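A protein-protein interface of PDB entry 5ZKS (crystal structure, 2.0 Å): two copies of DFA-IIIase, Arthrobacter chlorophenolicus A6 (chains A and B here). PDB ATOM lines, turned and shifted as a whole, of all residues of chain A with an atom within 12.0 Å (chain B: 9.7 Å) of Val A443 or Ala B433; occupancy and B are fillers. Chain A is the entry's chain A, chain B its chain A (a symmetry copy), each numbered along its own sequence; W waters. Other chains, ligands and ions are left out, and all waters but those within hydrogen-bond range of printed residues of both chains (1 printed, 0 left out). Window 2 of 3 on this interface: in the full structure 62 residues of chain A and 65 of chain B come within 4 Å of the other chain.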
ATOM      1  N   ASP A 402     -33.595  21.129 -14.217  1.00  0.00           N
ATOM      2  CA  ASP A 402     -33.974  21.376 -12.827  1.00  0.00           C
ATOM      3  C   ASP A 402     -35.342  22.070 -12.722  1.00  0.00           C
ATOM      4  O   ASP A 402     -35.833  22.670 -13.685  1.00  0.00           O
ATOM      5  CB  ASP A 402     -32.894  22.136 -12.058  1.00  0.00           C
ATOM      6  CG  ASP A 402     -32.934  21.839 -10.561  1.00  0.00           C
ATOM      7  OD1 ASP A 402     -33.883  21.146 -10.101  1.00  0.00           O
ATOM      8  OD2 ASP A 402     -32.017  22.292  -9.843  1.00  0.00           O
ATOM      9  N   ASP A 421     -33.905  21.317   8.128  1.00  0.00           N
ATOM     10  CA  ASP A 421     -33.177  20.597   7.091  1.00  0.00           C
ATOM     11  C   ASP A 421     -34.134  19.858   6.161  1.00  0.00           C
ATOM     12  O   ASP A 421     -33.985  18.659   5.907  1.00  0.00           O
ATOM     13  CB  ASP A 421     -32.197  19.590   7.716  1.00  0.00           C
ATOM     14  CG  ASP A 421     -31.262  20.216   8.710  1.00  0.00           C
ATOM     15  OD1 ASP A 421     -30.932  21.412   8.555  1.00  0.00           O
ATOM     16  OD2 ASP A 421     -30.853  19.505   9.659  1.00  0.00           O
ATOM     17  N   GLY A 423     -35.324  21.843   3.318  1.00  0.00           N
ATOM     18  CA  GLY A 423     -35.333  22.745   2.181  1.00  0.00           C
ATOM     19  C   GLY A 423     -34.526  23.994   2.491  1.00  0.00           C
ATOM     20  O   GLY A 423     -34.293  24.328   3.649  1.00  0.00           O
ATOM     21  N   SER A 424     -34.079  24.680   1.450  1.00  0.00           N
ATOM     22  CA  SER A 424     -33.400  25.958   1.621  1.00  0.00           C
ATOM     23  C   SER A 424     -34.443  26.999   2.020  1.00  0.00           C
ATOM     24  O   SER A 424     -35.638  26.702   2.005  1.00  0.00           O
ATOM     25  CB  SER A 424     -32.750  26.362   0.306  1.00  0.00           C
ATOM     26  OG  SER A 424     -33.750  26.553  -0.682  1.00  0.00           O
ATOM     27  N   ASP A 425     -34.007  28.212   2.353  1.00  0.00           N
ATOM     28  CA  ASP A 425     -34.941  29.281   2.743  1.00  0.00           C
ATOM     29  C   ASP A 425     -35.946  29.596   1.642  1.00  0.00           C
ATOM     30  O   ASP A 425     -37.129  29.775   1.927  1.00  0.00           O
ATOM     31  CB  ASP A 425     -34.211  30.559   3.203  1.00  0.00           C
ATOM     32  CG  ASP A 425     -33.784  30.496   4.668  1.00  0.00           C
ATOM     33  OD1 ASP A 425     -34.591  30.097   5.545  1.00  0.00           O
ATOM     34  OD2 ASP A 425     -32.625  30.847   4.953  1.00  0.00           O
ATOM     35  N   THR A 426     -35.495  29.643   0.389  1.00  0.00           N
ATOM     36  CA  THR A 426     -36.410  29.844  -0.741  1.00  0.00           C
ATOM     37  C   THR A 426     -37.446  28.720  -0.824  1.00  0.00           C
ATOM     38  O   THR A 426     -38.617  28.963  -1.145  1.00  0.00           O
ATOM     39  CB  THR A 426     -35.641  29.895  -2.077  1.00  0.00           C
ATOM     40  OG1 THR A 426     -34.578  30.840  -1.967  1.00  0.00           O
ATOM     41  CG2 THR A 426     -36.544  30.295  -3.217  1.00  0.00           C
ATOM     42  N   GLN A 427     -37.014  27.493  -0.529  1.00  0.00           N
ATOM     43  CA  GLN A 427     -37.892  26.317  -0.634  1.00  0.00           C
ATOM     44  C   GLN A 427     -38.891  26.163   0.498  1.00  0.00           C
ATOM     45  O   GLN A 427     -39.802  25.342   0.408  1.00  0.00           O
ATOM     46  CB  GLN A 427     -37.057  25.049  -0.697  1.00  0.00           C
ATOM     47  CG  GLN A 427     -36.335  24.873  -2.016  1.00  0.00           C
ATOM     48  CD  GLN A 427     -35.481  23.623  -2.049  1.00  0.00           C
ATOM     49  OE1 GLN A 427     -34.793  23.302  -1.082  1.00  0.00           O
ATOM     50  NE2 GLN A 427     -35.494  22.927  -3.179  1.00  0.00           N
ATOM     51  N   ALA A 439     -32.981  26.336   7.622  1.00  0.00           N
ATOM     52  CA  ALA A 439     -32.720  25.978   6.235  1.00  0.00           C
ATOM     53  C   ALA A 439     -31.667  24.896   6.162  1.00  0.00           C
ATOM     54  O   ALA A 439     -30.696  24.909   6.918  1.00  0.00           O
ATOM     55  CB  ALA A 439     -32.254  27.200   5.436  1.00  0.00           C
ATOM     56  N   THR A 440     -31.877  23.948   5.262  1.00  0.00           N
ATOM     57  CA  THR A 440     -30.821  23.031   4.868  1.00  0.00           C
ATOM     58  C   THR A 440     -29.637  23.861   4.390  1.00  0.00           C
ATOM     59  O   THR A 440     -29.820  24.740   3.539  1.00  0.00           O
ATOM     60  CB  THR A 440     -31.291  22.165   3.706  1.00  0.00           C
ATOM     61  OG1 THR A 440     -32.479  21.485   4.101  1.00  0.00           O
ATOM     62  CG2 THR A 440     -30.226  21.139   3.296  1.00  0.00           C
ATOM     63  N   PRO A 441     -28.435  23.615   4.939  1.00  0.00           N
ATOM     64  CA  PRO A 441     -27.265  24.338   4.435  1.00  0.00           C
ATOM     65  C   PRO A 441     -27.075  24.184   2.928  1.00  0.00           C
ATOM     66  O   PRO A 441     -27.367  23.117   2.374  1.00  0.00           O
ATOM     67  CB  PRO A 441     -26.112  23.684   5.188  1.00  0.00           C
ATOM     68  CG  PRO A 441     -26.718  23.297   6.494  1.00  0.00           C
ATOM     69  CD  PRO A 441     -28.124  22.874   6.177  1.00  0.00           C
ATOM     70  N   THR A 442     -26.609  25.244   2.277  1.00  0.00           N
ATOM     71  CA  THR A 442     -26.373  25.229   0.825  1.00  0.00           C
ATOM     72  C   THR A 442     -24.985  25.704   0.417  1.00  0.00           C
ATOM     73  O   THR A 442     -24.271  26.333   1.196  1.00  0.00           O
ATOM     74  CB  THR A 442     -27.348  26.166   0.088  1.00  0.00           C
ATOM     75  OG1 THR A 442     -27.530  27.359   0.857  1.00  0.00           O
ATOM     76  CG2 THR A 442     -28.692  25.485  -0.156  1.00  0.00           C
ATOM     77  N   VAL A 443     -24.627  25.373  -0.821  1.00  0.00           N
ATOM     78  CA  VAL A 443     -23.673  26.158  -1.612  1.00  0.00           C
ATOM     79  C   VAL A 443     -24.395  26.641  -2.869  1.00  0.00           C
ATOM     80  O   VAL A 443     -24.126  27.728  -3.376  1.00  0.00           O
ATOM     81  CB  VAL A 443     -22.420  25.359  -2.034  1.00  0.00           C
ATOM     82  CG1 VAL A 443     -21.425  25.284  -0.884  1.00  0.00           C
ATOM     83  CG2 VAL A 443     -22.787  23.969  -2.555  1.00  0.00           C
ATOM     84  N   GLY B 366     -25.844  15.775  -5.853  1.00  0.00           N
ATOM     85  CA  GLY B 366     -27.102  16.015  -5.173  1.00  0.00           C
ATOM     86  C   GLY B 366     -27.450  15.023  -4.085  1.00  0.00           C
ATOM     87  O   GLY B 366     -28.584  15.005  -3.624  1.00  0.00           O
ATOM     88  N   VAL B 410     -16.070  12.128  -0.010  1.00  0.00           N
ATOM     89  CA  VAL B 410     -16.626  12.590  -1.279  1.00  0.00           C
ATOM     90  C   VAL B 410     -15.488  12.754  -2.278  1.00  0.00           C
ATOM     91  O   VAL B 410     -14.688  13.696  -2.182  1.00  0.00           O
ATOM     92  CB  VAL B 410     -17.335  13.950  -1.128  1.00  0.00           C
ATOM     93  CG1 VAL B 410     -17.887  14.431  -2.469  1.00  0.00           C
ATOM     94  CG2 VAL B 410     -18.457  13.859  -0.107  1.00  0.00           C
ATOM     95  N   SER B 414     -17.584  13.453  -7.393  1.00  0.00           N
ATOM     96  CA  SER B 414     -18.936  13.668  -6.886  1.00  0.00           C
ATOM     97  C   SER B 414     -18.965  15.054  -6.275  1.00  0.00           C
ATOM     98  O   SER B 414     -18.024  15.444  -5.596  1.00  0.00           O
ATOM     99  CB  SER B 414     -19.319  12.588  -5.861  1.00  0.00           C
ATOM    100  OG  SER B 414     -20.626  12.793  -5.346  1.00  0.00           O
ATOM    101  N   ALA B 415     -20.023  15.813  -6.544  1.00  0.00           N
ATOM    102  CA  ALA B 415     -20.104  17.194  -6.079  1.00  0.00           C
ATOM    103  C   ALA B 415     -21.550  17.625  -5.848  1.00  0.00           C
ATOM    104  O   ALA B 415     -22.483  16.898  -6.208  1.00  0.00           O
ATOM    105  CB  ALA B 415     -19.420  18.119  -7.072  1.00  0.00           C
ATOM    106  N   ARG B 416     -21.716  18.797  -5.222  1.00  0.00           N
ATOM    107  CA  ARG B 416     -23.031  19.372  -4.929  1.00  0.00           C
ATOM    108  C   ARG B 416     -23.846  18.430  -4.045  1.00  0.00           C
ATOM    109  O   ARG B 416     -25.064  18.314  -4.189  1.00  0.00           O
ATOM    110  CB  ARG B 416     -23.789  19.682  -6.215  1.00  0.00           C
ATOM    111  CG  ARG B 416     -22.957  20.409  -7.258  1.00  0.00           C
ATOM    112  CD  ARG B 416     -22.955  21.914  -7.055  1.00  0.00           C
ATOM    113  NE  ARG B 416     -24.134  22.537  -7.657  1.00  0.00           N
ATOM    114  CZ  ARG B 416     -24.334  22.686  -8.965  1.00  0.00           C
ATOM    115  NH1 ARG B 416     -23.438  22.254  -9.853  1.00  0.00           N
ATOM    116  NH2 ARG B 416     -25.449  23.267  -9.397  1.00  0.00           N
ATOM    117  N   ASN B 417     -23.153  17.745  -3.148  1.00  0.00           N
ATOM    118  CA  ASN B 417     -23.795  16.916  -2.146  1.00  0.00           C
ATOM    119  C   ASN B 417     -24.017  17.732  -0.891  1.00  0.00           C
ATOM    120  O   ASN B 417     -23.431  18.801  -0.702  1.00  0.00           O
ATOM    121  CB  ASN B 417     -22.926  15.697  -1.834  1.00  0.00           C
ATOM    122  CG  ASN B 417     -22.605  14.876  -3.070  1.00  0.00           C
ATOM    123  OD1 ASN B 417     -23.484  14.243  -3.651  1.00  0.00           O
ATOM    124  ND2 ASN B 417     -21.327  14.859  -3.467  1.00  0.00           N
ATOM    125  N   THR B 418     -24.875  17.217  -0.026  1.00  0.00           N
ATOM    126  CA  THR B 418     -25.139  17.821   1.271  1.00  0.00           C
ATOM    127  C   THR B 418     -24.820  16.771   2.321  1.00  0.00           C
ATOM    128  O   THR B 418     -25.363  15.668   2.265  1.00  0.00           O
ATOM    129  CB  THR B 418     -26.604  18.252   1.341  1.00  0.00           C
ATOM    130  OG1 THR B 418     -26.871  19.115   0.239  1.00  0.00           O
ATOM    131  CG2 THR B 418     -26.917  18.979   2.645  1.00  0.00           C
ATOM    132  N   ILE B 419     -23.923  17.102   3.253  1.00  0.00           N
ATOM    133  CA  ILE B 419     -23.502  16.175   4.306  1.00  0.00           C
ATOM    134  C   ILE B 419     -23.730  16.830   5.664  1.00  0.00           C
ATOM    135  O   ILE B 419     -23.085  17.829   6.012  1.00  0.00           O
ATOM    136  CB  ILE B 419     -22.029  15.770   4.148  1.00  0.00           C
ATOM    137  CG1 ILE B 419     -21.793  15.219   2.737  1.00  0.00           C
ATOM    138  CG2 ILE B 419     -21.632  14.696   5.155  1.00  0.00           C
ATOM    139  CD1 ILE B 419     -20.416  15.506   2.220  1.00  0.00           C
ATOM    140  N   LEU B 420     -24.669  16.269   6.419  1.00  0.00           N
ATOM    141  CA  LEU B 420     -25.069  16.826   7.692  1.00  0.00           C
ATOM    142  C   LEU B 420     -24.952  15.806   8.803  1.00  0.00           C
ATOM    143  O   LEU B 420     -25.381  14.652   8.665  1.00  0.00           O
ATOM    144  CB  LEU B 420     -26.510  17.306   7.614  1.00  0.00           C
ATOM    145  CG  LEU B 420     -26.887  18.241   6.475  1.00  0.00           C
ATOM    146  CD1 LEU B 420     -28.366  18.542   6.612  1.00  0.00           C
ATOM    147  CD2 LEU B 420     -26.086  19.540   6.480  1.00  0.00           C
ATOM    148  N   ALA B 430     -14.036  16.083   2.101  1.00  0.00           N
ATOM    149  CA  ALA B 430     -14.861  16.620   1.042  1.00  0.00           C
ATOM    150  C   ALA B 430     -14.473  18.069   0.787  1.00  0.00           C
ATOM    151  O   ALA B 430     -14.085  18.794   1.712  1.00  0.00           O
ATOM    152  CB  ALA B 430     -16.333  16.555   1.439  1.00  0.00           C
ATOM    153  N   ASP B 431     -14.634  18.484  -0.464  1.00  0.00           N
ATOM    154  CA  ASP B 431     -14.390  19.852  -0.887  1.00  0.00           C
ATOM    155  C   ASP B 431     -15.556  20.721  -0.422  1.00  0.00           C
ATOM    156  O   ASP B 431     -16.663  20.647  -0.959  1.00  0.00           O
ATOM    157  CB  ASP B 431     -14.235  19.898  -2.410  1.00  0.00           C
ATOM    158  CG  ASP B 431     -13.857  21.268  -2.929  1.00  0.00           C
ATOM    159  OD1 ASP B 431     -13.920  22.257  -2.175  1.00  0.00           O
ATOM    160  OD2 ASP B 431     -13.514  21.362  -4.117  1.00  0.00           O
ATOM    161  N   ARG B 432     -15.292  21.538   0.592  1.00  0.00           N
ATOM    162  CA  ARG B 432     -16.306  22.423   1.165  1.00  0.00           C
ATOM    163  C   ARG B 432     -16.833  23.479   0.203  1.00  0.00           C
ATOM    164  O   ARG B 432     -17.894  24.037   0.452  1.00  0.00           O
ATOM    165  CB  ARG B 432     -15.778  23.110   2.431  1.00  0.00           C
ATOM    166  CG  ARG B 432     -16.064  22.358   3.721  1.00  0.00           C
ATOM    167  CD  ARG B 432     -15.367  21.010   3.798  1.00  0.00           C
ATOM    168  NE  ARG B 432     -15.532  20.393   5.115  1.00  0.00           N
ATOM    169  CZ  ARG B 432     -15.125  19.164   5.440  1.00  0.00           C
ATOM    170  NH1 ARG B 432     -14.523  18.385   4.546  1.00  0.00           N
ATOM    171  NH2 ARG B 432     -15.317  18.715   6.672  1.00  0.00           N
ATOM    172  N   ALA B 433     -16.100  23.767  -0.875  1.00  0.00           N
ATOM    173  CA  ALA B 433     -16.509  24.807  -1.831  1.00  0.00           C
ATOM    174  C   ALA B 433     -17.655  24.369  -2.752  1.00  0.00           C
ATOM    175  O   ALA B 433     -18.384  25.211  -3.274  1.00  0.00           O
ATOM    176  CB  ALA B 433     -15.314  25.268  -2.668  1.00  0.00           C
ATOM    177  N   VAL B 434     -17.803  23.061  -2.958  1.00  0.00           N
ATOM    178  CA  VAL B 434     -18.828  22.545  -3.861  1.00  0.00           C
ATOM    179  C   VAL B 434     -19.723  21.448  -3.250  1.00  0.00           C
ATOM    180  O   VAL B 434     -20.432  20.762  -3.983  1.00  0.00           O
ATOM    181  CB  VAL B 434     -18.205  22.036  -5.188  1.00  0.00           C
ATOM    182  CG1 VAL B 434     -17.568  23.183  -5.957  1.00  0.00           C
ATOM    183  CG2 VAL B 434     -17.199  20.910  -4.938  1.00  0.00           C
ATOM    184  N   ASN B 435     -19.682  21.297  -1.924  1.00  0.00           N
ATOM    185  CA  ASN B 435     -20.611  20.452  -1.161  1.00  0.00           C
ATOM    186  C   ASN B 435     -21.007  21.224   0.086  1.00  0.00           C
ATOM    187  O   ASN B 435     -20.163  21.924   0.657  1.00  0.00           O
ATOM    188  CB  ASN B 435     -19.937  19.155  -0.719  1.00  0.00           C
ATOM    189  CG  ASN B 435     -19.434  18.323  -1.880  1.00  0.00           C
ATOM    190  OD1 ASN B 435     -20.199  17.571  -2.491  1.00  0.00           O
ATOM    191  ND2 ASN B 435     -18.133  18.432  -2.180  1.00  0.00           N
ATOM    192  N   ALA B 436     -22.258  21.097   0.527  1.00  0.00           N
ATOM    193  CA  ALA B 436     -22.699  21.735   1.768  1.00  0.00           C
ATOM    194  C   ALA B 436     -22.443  20.780   2.929  1.00  0.00           C
ATOM    195  O   ALA B 436     -23.074  19.725   3.009  1.00  0.00           O
ATOM    196  CB  ALA B 436     -24.174  22.100   1.687  1.00  0.00           C
ATOM    197  N   ILE B 437     -21.500  21.141   3.804  1.00  0.00           N
ATOM    198  CA  ILE B 437     -21.083  20.274   4.903  1.00  0.00           C
ATOM    199  C   ILE B 437     -21.387  20.908   6.259  1.00  0.00           C
ATOM    200  O   ILE B 437     -20.982  22.034   6.531  1.00  0.00           O
ATOM    201  CB  ILE B 437     -19.582  19.927   4.828  1.00  0.00           C
ATOM    202  CG1 ILE B 437     -19.299  18.991   3.646  1.00  0.00           C
ATOM    203  CG2 ILE B 437     -19.124  19.208   6.090  1.00  0.00           C
ATOM    204  CD1 ILE B 437     -18.574  19.650   2.516  1.00  0.00           C
ATOM    205  N   ARG B 438     -22.107  20.177   7.102  1.00  0.00           N
ATOM    206  CA  ARG B 438     -22.248  20.543   8.507  1.00  0.00           C
ATOM    207  C   ARG B 438     -21.688  19.419   9.363  1.00  0.00           C
ATOM    208  O   ARG B 438     -22.216  18.304   9.362  1.00  0.00           O
ATOM    209  CB  ARG B 438     -23.701  20.812   8.890  1.00  0.00           C
ATOM    210  CG  ARG B 438     -23.856  21.247  10.348  1.00  0.00           C
ATOM    211  CD  ARG B 438     -25.280  21.645  10.679  1.00  0.00           C
ATOM    212  NE  ARG B 438     -26.192  20.504  10.773  1.00  0.00           N
ATOM    213  CZ  ARG B 438     -27.437  20.481  10.295  1.00  0.00           C
ATOM    214  NH1 ARG B 438     -27.943  21.513   9.622  1.00  0.00           N
ATOM    215  NH2 ARG B 438     -28.175  19.401  10.460  1.00  0.00           N
HETATM  216  O   HOH W   1     -27.749  21.840   0.177  1.00  0.00           O
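OD2 of Asp A421 is in salt-bridge range of NH2 of Arg B438.
N of Arg B416 lies within hydrogen-bond range of OD1 of Asn B435 (3.4 Å).
The side-chain carboxylate (OD1) of Asp B431 lies within hydrogen-bond range of the backbone NH (N) of Ala B433 (3.0 Å).
O of Ile B419 lies within hydrogen-bond range of N of Arg B438 (2.8 Å).
The backbone carbonyl oxygen of Ala B430 sits at hydrogen-bond distance from the guanidinium group of Arg B432 (2.9 Å).
The side-chain amide nitrogen (ND2) of Asn B435 is in hydrogen-bond range of the backbone carbonyl oxygen (O) of Asp B431, at 2.9 Å.
N of Ala B436 is in hydrogen-bond range of O of Asn B417, 2.9 Å away.
CG of Asp A421 touches CD1 of Leu B420, at 3.9 Å.
CD2 of Leu B420 touches CG of Pro A441, at 3.8 Å.
CB of Ala B436 touches O of Pro A441, 3.4 Å away.
Arg B438 touches Pro A441.
Thr A442 touches Ala B436.
Val A443 touches Arg B432.
CG1 of Val A443 touches O of Ala B433, 3.9 Å away.
Val A443 touches Asn B435.
Of the printed residues of chain B, Asp A421 touches Leu B420 (3.9 Å) and Arg B438 (2.8 Å).
Ala A439 touches none of the printed residues of chain B.
Of chain B, only Ala B436 comes within 4 Å of Thr A442.
Of chain B, only Arg B432, Ala B433 and Asn B435 come within 4 Å of Val A443.
Ser B414 touches none of the printed residues of chain A.
Of the printed residues of chain A, Leu B420 touches Asp A421 (3.9 Å) and Pro A441 (3.8 Å).
No residue of chain A comes within 4 Å of Asp B431.
Of chain A, only Val A443 comes within 4 Å of Ala B433.
No residue of chain A comes within 4 Å of Val B434.
Asn B435 touches one residue of chain A.
Of chain A, only Pro A441 and Thr A442 come within 4 Å of Ala B436.
Of the printed residues of chain A, Arg B438 touches Asp A421 and Pro A441.
The nearest residue of chain B that does not touch Val A443 is Val B434 (4.03 Å).
The nearest residue of chain A that does not touch Ala B433 is Thr A442 (7.5 Å).
Printed residues of chain B that touch a printed residue of chain A: Leu B420, Arg B432, Ala B433, Asn B435, Ala B436 and Arg B438.
Hydrophobic or aromatic side chains of chain B within 4 Å of the printed part of chain A: Leu B420 and Ala B436.
Hydrophobic or aromatic side chains of chain A that line the printed part of chain B: Pro A441 and Val A443.
Among the printed residues, 9 pairs touch across the chains.
Among the printed residues, Asp or Glu carboxylates within 4 Å of a Lys or Arg side-chain nitrogen of the other chain: Asp A421 with Arg B438 (2.8 Å).
No position is printed for both chains.
Water W1 lies within hydrogen-bond range of O of Pro A441 (2.6 Å) and OG1 of Thr B418 (2.9 Å).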
